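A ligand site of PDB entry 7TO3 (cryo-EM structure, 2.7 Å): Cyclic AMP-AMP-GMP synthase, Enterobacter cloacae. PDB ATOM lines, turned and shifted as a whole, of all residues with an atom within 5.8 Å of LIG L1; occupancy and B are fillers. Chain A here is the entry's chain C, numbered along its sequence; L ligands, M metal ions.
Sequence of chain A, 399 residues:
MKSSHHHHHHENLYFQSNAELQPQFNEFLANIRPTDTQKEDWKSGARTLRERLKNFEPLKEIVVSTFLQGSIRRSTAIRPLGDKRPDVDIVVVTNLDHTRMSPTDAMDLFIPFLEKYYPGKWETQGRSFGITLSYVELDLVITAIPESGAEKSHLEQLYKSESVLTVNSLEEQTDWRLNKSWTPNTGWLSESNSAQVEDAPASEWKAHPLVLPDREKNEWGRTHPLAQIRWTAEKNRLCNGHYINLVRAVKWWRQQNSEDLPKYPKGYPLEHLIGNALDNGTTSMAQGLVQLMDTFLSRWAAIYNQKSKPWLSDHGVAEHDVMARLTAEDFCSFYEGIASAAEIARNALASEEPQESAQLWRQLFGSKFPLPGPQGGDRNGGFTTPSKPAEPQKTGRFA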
ATOM      1  N   GLN A  69     -10.354 -16.440 -32.872  1.00  0.00           N
ATOM      2  CA  GLN A  69     -10.161 -17.525 -31.918  1.00  0.00           C
ATOM      3  C   GLN A  69     -10.185 -18.872 -32.636  1.00  0.00           C
ATOM      4  O   GLN A  69     -10.137 -18.928 -33.863  1.00  0.00           O
ATOM      5  CB  GLN A  69     -11.244 -17.488 -30.835  1.00  0.00           C
ATOM      6  CG  GLN A  69     -12.621 -17.889 -31.339  1.00  0.00           C
ATOM      7  CD  GLN A  69     -13.655 -17.953 -30.227  1.00  0.00           C
ATOM      8  OE1 GLN A  69     -13.378 -17.583 -29.089  1.00  0.00           O
ATOM      9  NE2 GLN A  69     -14.845 -18.436 -30.563  1.00  0.00           N
ATOM     10  N   ASP A  89     -12.953 -18.983 -36.846  1.00  0.00           N
ATOM     11  CA  ASP A  89     -13.818 -18.549 -35.759  1.00  0.00           C
ATOM     12  C   ASP A  89     -13.454 -17.140 -35.304  1.00  0.00           C
ATOM     13  O   ASP A  89     -12.295 -16.855 -34.990  1.00  0.00           O
ATOM     14  CB  ASP A  89     -13.718 -19.520 -34.580  1.00  0.00           C
ATOM     15  CG  ASP A  89     -14.125 -20.930 -34.945  1.00  0.00           C
ATOM     16  OD1 ASP A  89     -15.326 -21.146 -35.241  1.00  0.00           O
ATOM     17  OD2 ASP A  89     -13.259 -21.825 -34.953  1.00  0.00           O
ATOM     18  N   VAL A  91     -14.979 -13.630 -32.892  1.00  0.00           N
ATOM     19  CA  VAL A  91     -15.848 -13.218 -31.800  1.00  0.00           C
ATOM     20  C   VAL A  91     -15.948 -11.705 -31.787  1.00  0.00           C
ATOM     21  O   VAL A  91     -14.927 -10.999 -31.861  1.00  0.00           O
ATOM     22  CB  VAL A  91     -15.335 -13.730 -30.441  1.00  0.00           C
ATOM     23  CG1 VAL A  91     -16.008 -12.984 -29.296  1.00  0.00           C
ATOM     24  CG2 VAL A  91     -15.604 -15.215 -30.313  1.00  0.00           C
ATOM     25  N   ARG A 127     -26.219 -20.627 -33.160  1.00  0.00           N
ATOM     26  CA  ARG A 127     -25.863 -19.441 -32.393  1.00  0.00           C
ATOM     27  C   ARG A 127     -24.946 -18.490 -33.155  1.00  0.00           C
ATOM     28  O   ARG A 127     -24.523 -17.489 -32.579  1.00  0.00           O
ATOM     29  CB  ARG A 127     -25.180 -19.857 -31.083  1.00  0.00           C
ATOM     30  CG  ARG A 127     -23.757 -20.361 -31.263  1.00  0.00           C
ATOM     31  CD  ARG A 127     -23.129 -20.759 -29.942  1.00  0.00           C
ATOM     32  NE  ARG A 127     -23.665 -22.019 -29.425  1.00  0.00           N
ATOM     33  CZ  ARG A 127     -23.240 -22.619 -28.330  1.00  0.00           C
ATOM     34  NH1 ARG A 127     -22.258 -22.106 -27.600  1.00  0.00           N
ATOM     35  NH2 ARG A 127     -23.799 -23.766 -27.954  1.00  0.00           N
ATOM     36  N   ASP A 139     -16.964 -17.778 -39.189  1.00  0.00           N
ATOM     37  CA  ASP A 139     -18.028 -18.113 -38.255  1.00  0.00           C
ATOM     38  C   ASP A 139     -17.922 -17.154 -37.072  1.00  0.00           C
ATOM     39  O   ASP A 139     -16.980 -17.241 -36.282  1.00  0.00           O
ATOM     40  CB  ASP A 139     -17.936 -19.571 -37.794  1.00  0.00           C
ATOM     41  CG  ASP A 139     -19.246 -20.088 -37.222  1.00  0.00           C
ATOM     42  OD1 ASP A 139     -20.315 -19.690 -37.727  1.00  0.00           O
ATOM     43  OD2 ASP A 139     -19.196 -20.894 -36.273  1.00  0.00           O
ATOM     44  N   VAL A 141     -19.632 -15.065 -33.672  1.00  0.00           N
ATOM     45  CA  VAL A 141     -20.527 -15.211 -32.537  1.00  0.00           C
ATOM     46  C   VAL A 141     -20.578 -13.882 -31.798  1.00  0.00           C
ATOM     47  O   VAL A 141     -19.545 -13.248 -31.572  1.00  0.00           O
ATOM     48  CB  VAL A 141     -20.079 -16.347 -31.593  1.00  0.00           C
ATOM     49  CG1 VAL A 141     -21.041 -16.482 -30.426  1.00  0.00           C
ATOM     50  CG2 VAL A 141     -19.952 -17.657 -32.353  1.00  0.00           C
ATOM     51  N   LEU A 212     -22.464 -15.676 -23.914  1.00  0.00           N
ATOM     52  CA  LEU A 212     -22.691 -15.980 -25.319  1.00  0.00           C
ATOM     53  C   LEU A 212     -24.004 -16.732 -25.462  1.00  0.00           C
ATOM     54  O   LEU A 212     -24.478 -17.358 -24.509  1.00  0.00           O
ATOM     55  CB  LEU A 212     -21.542 -16.804 -25.919  1.00  0.00           C
ATOM     56  CG  LEU A 212     -21.503 -18.302 -25.622  1.00  0.00           C
ATOM     57  CD1 LEU A 212     -20.547 -19.003 -26.573  1.00  0.00           C
ATOM     58  CD2 LEU A 212     -21.127 -18.597 -24.180  1.00  0.00           C
ATOM     59  N   PRO A 213     -24.621 -16.684 -26.646  1.00  0.00           N
ATOM     60  CA  PRO A 213     -25.871 -17.429 -26.847  1.00  0.00           C
ATOM     61  C   PRO A 213     -25.637 -18.935 -26.879  1.00  0.00           C
ATOM     62  O   PRO A 213     -24.526 -19.418 -27.107  1.00  0.00           O
ATOM     63  CB  PRO A 213     -26.372 -16.924 -28.207  1.00  0.00           C
ATOM     64  CG  PRO A 213     -25.633 -15.643 -28.450  1.00  0.00           C
ATOM     65  CD  PRO A 213     -24.295 -15.852 -27.809  1.00  0.00           C
ATOM     66  N   ASP A 214     -26.720 -19.674 -26.635  1.00  0.00           N
ATOM     67  CA  ASP A 214     -26.694 -21.132 -26.669  1.00  0.00           C
ATOM     68  C   ASP A 214     -27.126 -21.636 -28.044  1.00  0.00           C
ATOM     69  O   ASP A 214     -27.318 -20.865 -28.986  1.00  0.00           O
ATOM     70  CB  ASP A 214     -27.562 -21.717 -25.561  1.00  0.00           C
ATOM     71  CG  ASP A 214     -26.945 -21.561 -24.186  1.00  0.00           C
ATOM     72  OD1 ASP A 214     -25.778 -21.123 -24.099  1.00  0.00           O
ATOM     73  OD2 ASP A 214     -27.633 -21.875 -23.189  1.00  0.00           O
ATOM     74  N   ARG A 215     -27.292 -22.961 -28.157  1.00  0.00           N
ATOM     75  CA  ARG A 215     -27.684 -23.549 -29.431  1.00  0.00           C
ATOM     76  C   ARG A 215     -29.055 -23.081 -29.878  1.00  0.00           C
ATOM     77  O   ARG A 215     -29.260 -22.767 -31.065  1.00  0.00           O
ATOM     78  CB  ARG A 215     -27.655 -25.084 -29.330  1.00  0.00           C
ATOM     79  CG  ARG A 215     -26.315 -25.666 -28.940  1.00  0.00           C
ATOM     80  CD  ARG A 215     -25.473 -25.987 -30.167  1.00  0.00           C
ATOM     81  NE  ARG A 215     -24.260 -26.722 -29.821  1.00  0.00           N
ATOM     82  CZ  ARG A 215     -24.177 -28.048 -29.782  1.00  0.00           C
ATOM     83  NH1 ARG A 215     -25.220 -28.816 -30.078  1.00  0.00           N
ATOM     84  NH2 ARG A 215     -23.024 -28.618 -29.459  1.00  0.00           N
ATOM     85  N   GLY A 221     -25.071 -18.486 -21.940  1.00  0.00           N
ATOM     86  CA  GLY A 221     -24.086 -19.256 -21.236  1.00  0.00           C
ATOM     87  C   GLY A 221     -22.763 -18.529 -21.116  1.00  0.00           C
ATOM     88  O   GLY A 221     -22.610 -17.384 -21.577  1.00  0.00           O
ATOM     89  N   ARG A 222     -21.785 -19.199 -20.531  1.00  0.00           N
ATOM     90  CA  ARG A 222     -20.502 -18.594 -20.198  1.00  0.00           C
ATOM     91  C   ARG A 222     -19.395 -19.199 -21.043  1.00  0.00           C
ATOM     92  O   ARG A 222     -19.365 -20.411 -21.274  1.00  0.00           O
ATOM     93  CB  ARG A 222     -20.187 -18.779 -18.714  1.00  0.00           C
ATOM     94  CG  ARG A 222     -21.163 -18.087 -17.780  1.00  0.00           C
ATOM     95  CD  ARG A 222     -20.706 -18.151 -16.337  1.00  0.00           C
ATOM     96  NE  ARG A 222     -20.368 -19.508 -15.942  1.00  0.00           N
ATOM     97  CZ  ARG A 222     -21.213 -20.366 -15.393  1.00  0.00           C
ATOM     98  NH1 ARG A 222     -22.467 -20.035 -15.155  1.00  0.00           N
ATOM     99  NH2 ARG A 222     -20.791 -21.577 -15.063  1.00  0.00           N
ATOM    100  N   THR A 223     -18.486 -18.341 -21.517  1.00  0.00           N
ATOM    101  CA  THR A 223     -17.310 -18.765 -22.268  1.00  0.00           C
ATOM    102  C   THR A 223     -16.128 -17.893 -21.866  1.00  0.00           C
ATOM    103  O   THR A 223     -16.310 -16.786 -21.336  1.00  0.00           O
ATOM    104  CB  THR A 223     -17.520 -18.682 -23.784  1.00  0.00           C
ATOM    105  OG1 THR A 223     -16.395 -19.251 -24.454  1.00  0.00           O
ATOM    106  CG2 THR A 223     -17.688 -17.241 -24.224  1.00  0.00           C
ATOM    107  N   HIS A 224     -14.926 -18.389 -22.118  1.00  0.00           N
ATOM    108  CA  HIS A 224     -13.684 -17.698 -21.744  1.00  0.00           C
ATOM    109  C   HIS A 224     -12.546 -18.235 -22.616  1.00  0.00           C
ATOM    110  O   HIS A 224     -11.856 -19.188 -22.235  1.00  0.00           O
ATOM    111  CB  HIS A 224     -13.393 -17.869 -20.259  1.00  0.00           C
ATOM    112  CG  HIS A 224     -12.302 -16.996 -19.743  1.00  0.00           C
ATOM    113  ND1 HIS A 224     -12.361 -15.628 -19.762  1.00  0.00           N
ATOM    114  CD2 HIS A 224     -11.112 -17.309 -19.172  1.00  0.00           C
ATOM    115  CE1 HIS A 224     -11.264 -15.118 -19.238  1.00  0.00           C
ATOM    116  NE2 HIS A 224     -10.481 -16.121 -18.877  1.00  0.00           N
ATOM    117  N   PRO A 225     -12.336 -17.649 -23.790  1.00  0.00           N
ATOM    118  CA  PRO A 225     -11.348 -18.221 -24.718  1.00  0.00           C
ATOM    119  C   PRO A 225      -9.916 -17.785 -24.449  1.00  0.00           C
ATOM    120  O   PRO A 225      -8.974 -18.512 -24.812  1.00  0.00           O
ATOM    121  CB  PRO A 225     -11.836 -17.722 -26.092  1.00  0.00           C
ATOM    122  CG  PRO A 225     -12.497 -16.417 -25.781  1.00  0.00           C
ATOM    123  CD  PRO A 225     -13.124 -16.573 -24.415  1.00  0.00           C
ATOM    124  N   HIS A 320     -17.668 -26.186 -15.721  1.00  0.00           N
ATOM    125  CA  HIS A 320     -18.184 -26.792 -16.934  1.00  0.00           C
ATOM    126  C   HIS A 320     -17.402 -28.056 -17.275  1.00  0.00           C
ATOM    127  O   HIS A 320     -16.242 -28.210 -16.897  1.00  0.00           O
ATOM    128  CB  HIS A 320     -18.116 -25.812 -18.115  1.00  0.00           C
ATOM    129  CG  HIS A 320     -19.183 -24.769 -18.100  1.00  0.00           C
ATOM    130  ND1 HIS A 320     -19.123 -23.622 -18.867  1.00  0.00           N
ATOM    131  CD2 HIS A 320     -20.339 -24.683 -17.409  1.00  0.00           C
ATOM    132  CE1 HIS A 320     -20.194 -22.882 -18.647  1.00  0.00           C
ATOM    133  NE2 HIS A 320     -20.948 -23.502 -17.762  1.00  0.00           N
ATOM    134  N   ARG A 325     -21.356 -33.696 -23.797  1.00  0.00           N
ATOM    135  CA  ARG A 325     -22.225 -34.232 -24.828  1.00  0.00           C
ATOM    136  C   ARG A 325     -21.687 -35.517 -25.451  1.00  0.00           C
ATOM    137  O   ARG A 325     -22.158 -35.926 -26.514  1.00  0.00           O
ATOM    138  CB  ARG A 325     -22.444 -33.182 -25.922  1.00  0.00           C
ATOM    139  CG  ARG A 325     -23.355 -32.029 -25.501  1.00  0.00           C
ATOM    140  CD  ARG A 325     -23.465 -30.973 -26.580  1.00  0.00           C
ATOM    141  NE  ARG A 325     -24.505 -30.006 -26.293  1.00  0.00           N
ATOM    142  CZ  ARG A 325     -25.743 -30.062 -26.761  1.00  0.00           C
ATOM    143  NH1 ARG A 325     -26.134 -31.039 -27.560  1.00  0.00           N
ATOM    144  NH2 ARG A 325     -26.617 -29.116 -26.422  1.00  0.00           N
HETATM  145  P1  LIG L   1     -24.503 -25.899 -25.099  1.00  0.00           P
HETATM  146  O1  LIG L   1     -24.259 -24.508 -25.616  1.00  0.00           O
HETATM  147  O2  LIG L   1     -25.162 -26.836 -26.098  1.00  0.00           O
HETATM  148  O3  LIG L   1     -25.090 -25.955 -23.706  1.00  0.00           O
HETATM  149  P2  LIG L   1     -22.034 -26.702 -26.163  1.00  0.00           P
HETATM  150  O4  LIG L   1     -22.652 -26.157 -27.419  1.00  0.00           O
HETATM  151  O5  LIG L   1     -21.488 -28.115 -26.136  1.00  0.00           O
HETATM  152  O6  LIG L   1     -23.029 -26.506 -24.915  1.00  0.00           O
HETATM  153  O7  LIG L   1     -20.849 -25.695 -25.740  1.00  0.00           O
HETATM  154  C1  LIG L   1     -19.717 -26.149 -24.995  1.00  0.00           C
HETATM  155  C2  LIG L   1     -19.004 -24.912 -24.469  1.00  0.00           C
HETATM  156  O8  LIG L   1     -18.150 -24.378 -25.483  1.00  0.00           O
HETATM  157  C3  LIG L   1     -19.987 -23.829 -24.088  1.00  0.00           C
HETATM  158  O9  LIG L   1     -19.973 -23.613 -22.677  1.00  0.00           O
HETATM  159  C4  LIG L   1     -19.539 -22.570 -24.817  1.00  0.00           C
HETATM  160  O10 LIG L   1     -19.229 -21.545 -23.869  1.00  0.00           O
HETATM  161  C5  LIG L   1     -18.289 -22.964 -25.596  1.00  0.00           C
HETATM  162  N1  LIG L   1     -18.444 -22.611 -27.025  1.00  0.00           N
HETATM  163  C6  LIG L   1     -19.125 -23.315 -27.938  1.00  0.00           C
HETATM  164  N2  LIG L   1     -19.081 -22.721 -29.159  1.00  0.00           N
HETATM  165  C7  LIG L   1     -18.331 -21.613 -29.034  1.00  0.00           C
HETATM  166  C8  LIG L   1     -17.876 -20.520 -29.935  1.00  0.00           C
HETATM  167  N3  LIG L   1     -18.223 -20.514 -31.247  1.00  0.00           N
HETATM  168  N4  LIG L   1     -17.116 -19.542 -29.403  1.00  0.00           N
HETATM  169  C9  LIG L   1     -16.775 -19.543 -28.098  1.00  0.00           C
HETATM  170  N5  LIG L   1     -17.154 -20.490 -27.227  1.00  0.00           N
HETATM  171  C10 LIG L   1     -17.924 -21.538 -27.624  1.00  0.00           C
HETATM  172  P1  LG2 L   2     -12.025 -27.530 -35.848  1.00  0.00           P
HETATM  173  O1  LG2 L   2     -11.749 -26.392 -36.764  1.00  0.00           O
HETATM  174  O2  LG2 L   2     -13.050 -28.529 -36.394  1.00  0.00           O
HETATM  175  O3  LG2 L   2     -10.766 -28.281 -35.408  1.00  0.00           O
HETATM  176  P2  LG2 L   2     -12.367 -25.984 -33.298  1.00  0.00           P
HETATM  177  O4  LG2 L   2     -11.244 -26.436 -32.447  1.00  0.00           O
HETATM  178  O5  LG2 L   2     -12.200 -24.603 -33.928  1.00  0.00           O
HETATM  179  O6  LG2 L   2     -12.672 -27.004 -34.473  1.00  0.00           O
HETATM  180  P3  LG2 L   2     -15.209 -25.376 -32.729  1.00  0.00           P
HETATM  181  O7  LG2 L   2     -15.307 -24.648 -34.010  1.00  0.00           O
HETATM  182  O8  LG2 L   2     -16.197 -26.538 -32.583  1.00  0.00           O
HETATM  183  O9  LG2 L   2     -13.743 -25.983 -32.510  1.00  0.00           O
HETATM  184  O10 LG2 L   2     -15.380 -24.419 -31.493  1.00  0.00           O
HETATM  185  C1  LG2 L   2     -14.885 -23.063 -31.525  1.00  0.00           C
HETATM  186  C2  LG2 L   2     -14.307 -22.731 -30.171  1.00  0.00           C
HETATM  187  O11 LG2 L   2     -15.322 -22.862 -29.157  1.00  0.00           O
HETATM  188  C3  LG2 L   2     -13.168 -23.636 -29.712  1.00  0.00           C
HETATM  189  O12 LG2 L   2     -11.917 -23.178 -30.201  1.00  0.00           O
HETATM  190  C4  LG2 L   2     -13.264 -23.513 -28.182  1.00  0.00           C
HETATM  191  O13 LG2 L   2     -12.617 -22.336 -27.709  1.00  0.00           O
HETATM  192  C5  LG2 L   2     -14.773 -23.415 -27.977  1.00  0.00           C
HETATM  193  N1  LG2 L   2     -15.426 -24.701 -27.721  1.00  0.00           N
HETATM  194  C6  LG2 L   2     -16.075 -25.492 -28.640  1.00  0.00           C
HETATM  195  N2  LG2 L   2     -16.573 -26.599 -28.135  1.00  0.00           N
HETATM  196  C7  LG2 L   2     -16.212 -26.535 -26.794  1.00  0.00           C
HETATM  197  C8  LG2 L   2     -16.435 -27.403 -25.705  1.00  0.00           C
HETATM  198  N3  LG2 L   2     -17.097 -28.555 -25.799  1.00  0.00           N
HETATM  199  N4  LG2 L   2     -15.948 -27.035 -24.496  1.00  0.00           N
HETATM  200  C9  LG2 L   2     -15.286 -25.883 -24.402  1.00  0.00           C
HETATM  201  N5  LG2 L   2     -15.014 -24.983 -25.341  1.00  0.00           N
HETATM  202  C10 LG2 L   2     -15.502 -25.365 -26.531  1.00  0.00           C
HETATM  203 MG    MG M   1     -16.717 -23.424 -36.009  1.00  0.00          MG
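O of Asp 89 sits at hydrogen-bond distance from N of Gln 69, at 2.9 Å. A ring nitrogen (NE2) of His 320 is in hydrogen-bond range of the guanidinium group of Arg 222, at 3.3 Å. The backbone carbonyl oxygen of Leu 212 is in hydrogen-bond range of the backbone NH of Gly 221, at 2.9 Å.
Val 141 touches LIG L1 (CG2 to N3, 3.5 Å). Leu 212 touches LIG L1 (CD2 to O10, 3.5 Å). His 320 touches LIG L1. Hydrophobic or aromatic side chains that line LIG L1: Val 141 and Leu 212. Of the 17 residues printed, 9 come within 4 Å of LIG L1.
N4 of LIG L1 is in hydrogen-bond range of NE2 of Gln 69 (2.8 Å). NH2 of Arg 127 lies within salt-bridge range of O1 of LIG L1, at 2.5 Å. An oxygen (O10) of LIG L1 lies within hydrogen-bond range of the backbone carbonyl oxygen (O) of Arg 222 (2.8 Å). An oxygen (O2) of LIG L1 is in salt-bridge range of the guanidinium group of Arg 325. OG1 of Thr 223 is in hydrogen-bond range of N5 of LIG L1 (3.1 Å). An oxygen (O4) of LIG L1 is in salt-bridge range of the guanidinium group (NE) of Arg 215, 2.9 Å away.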
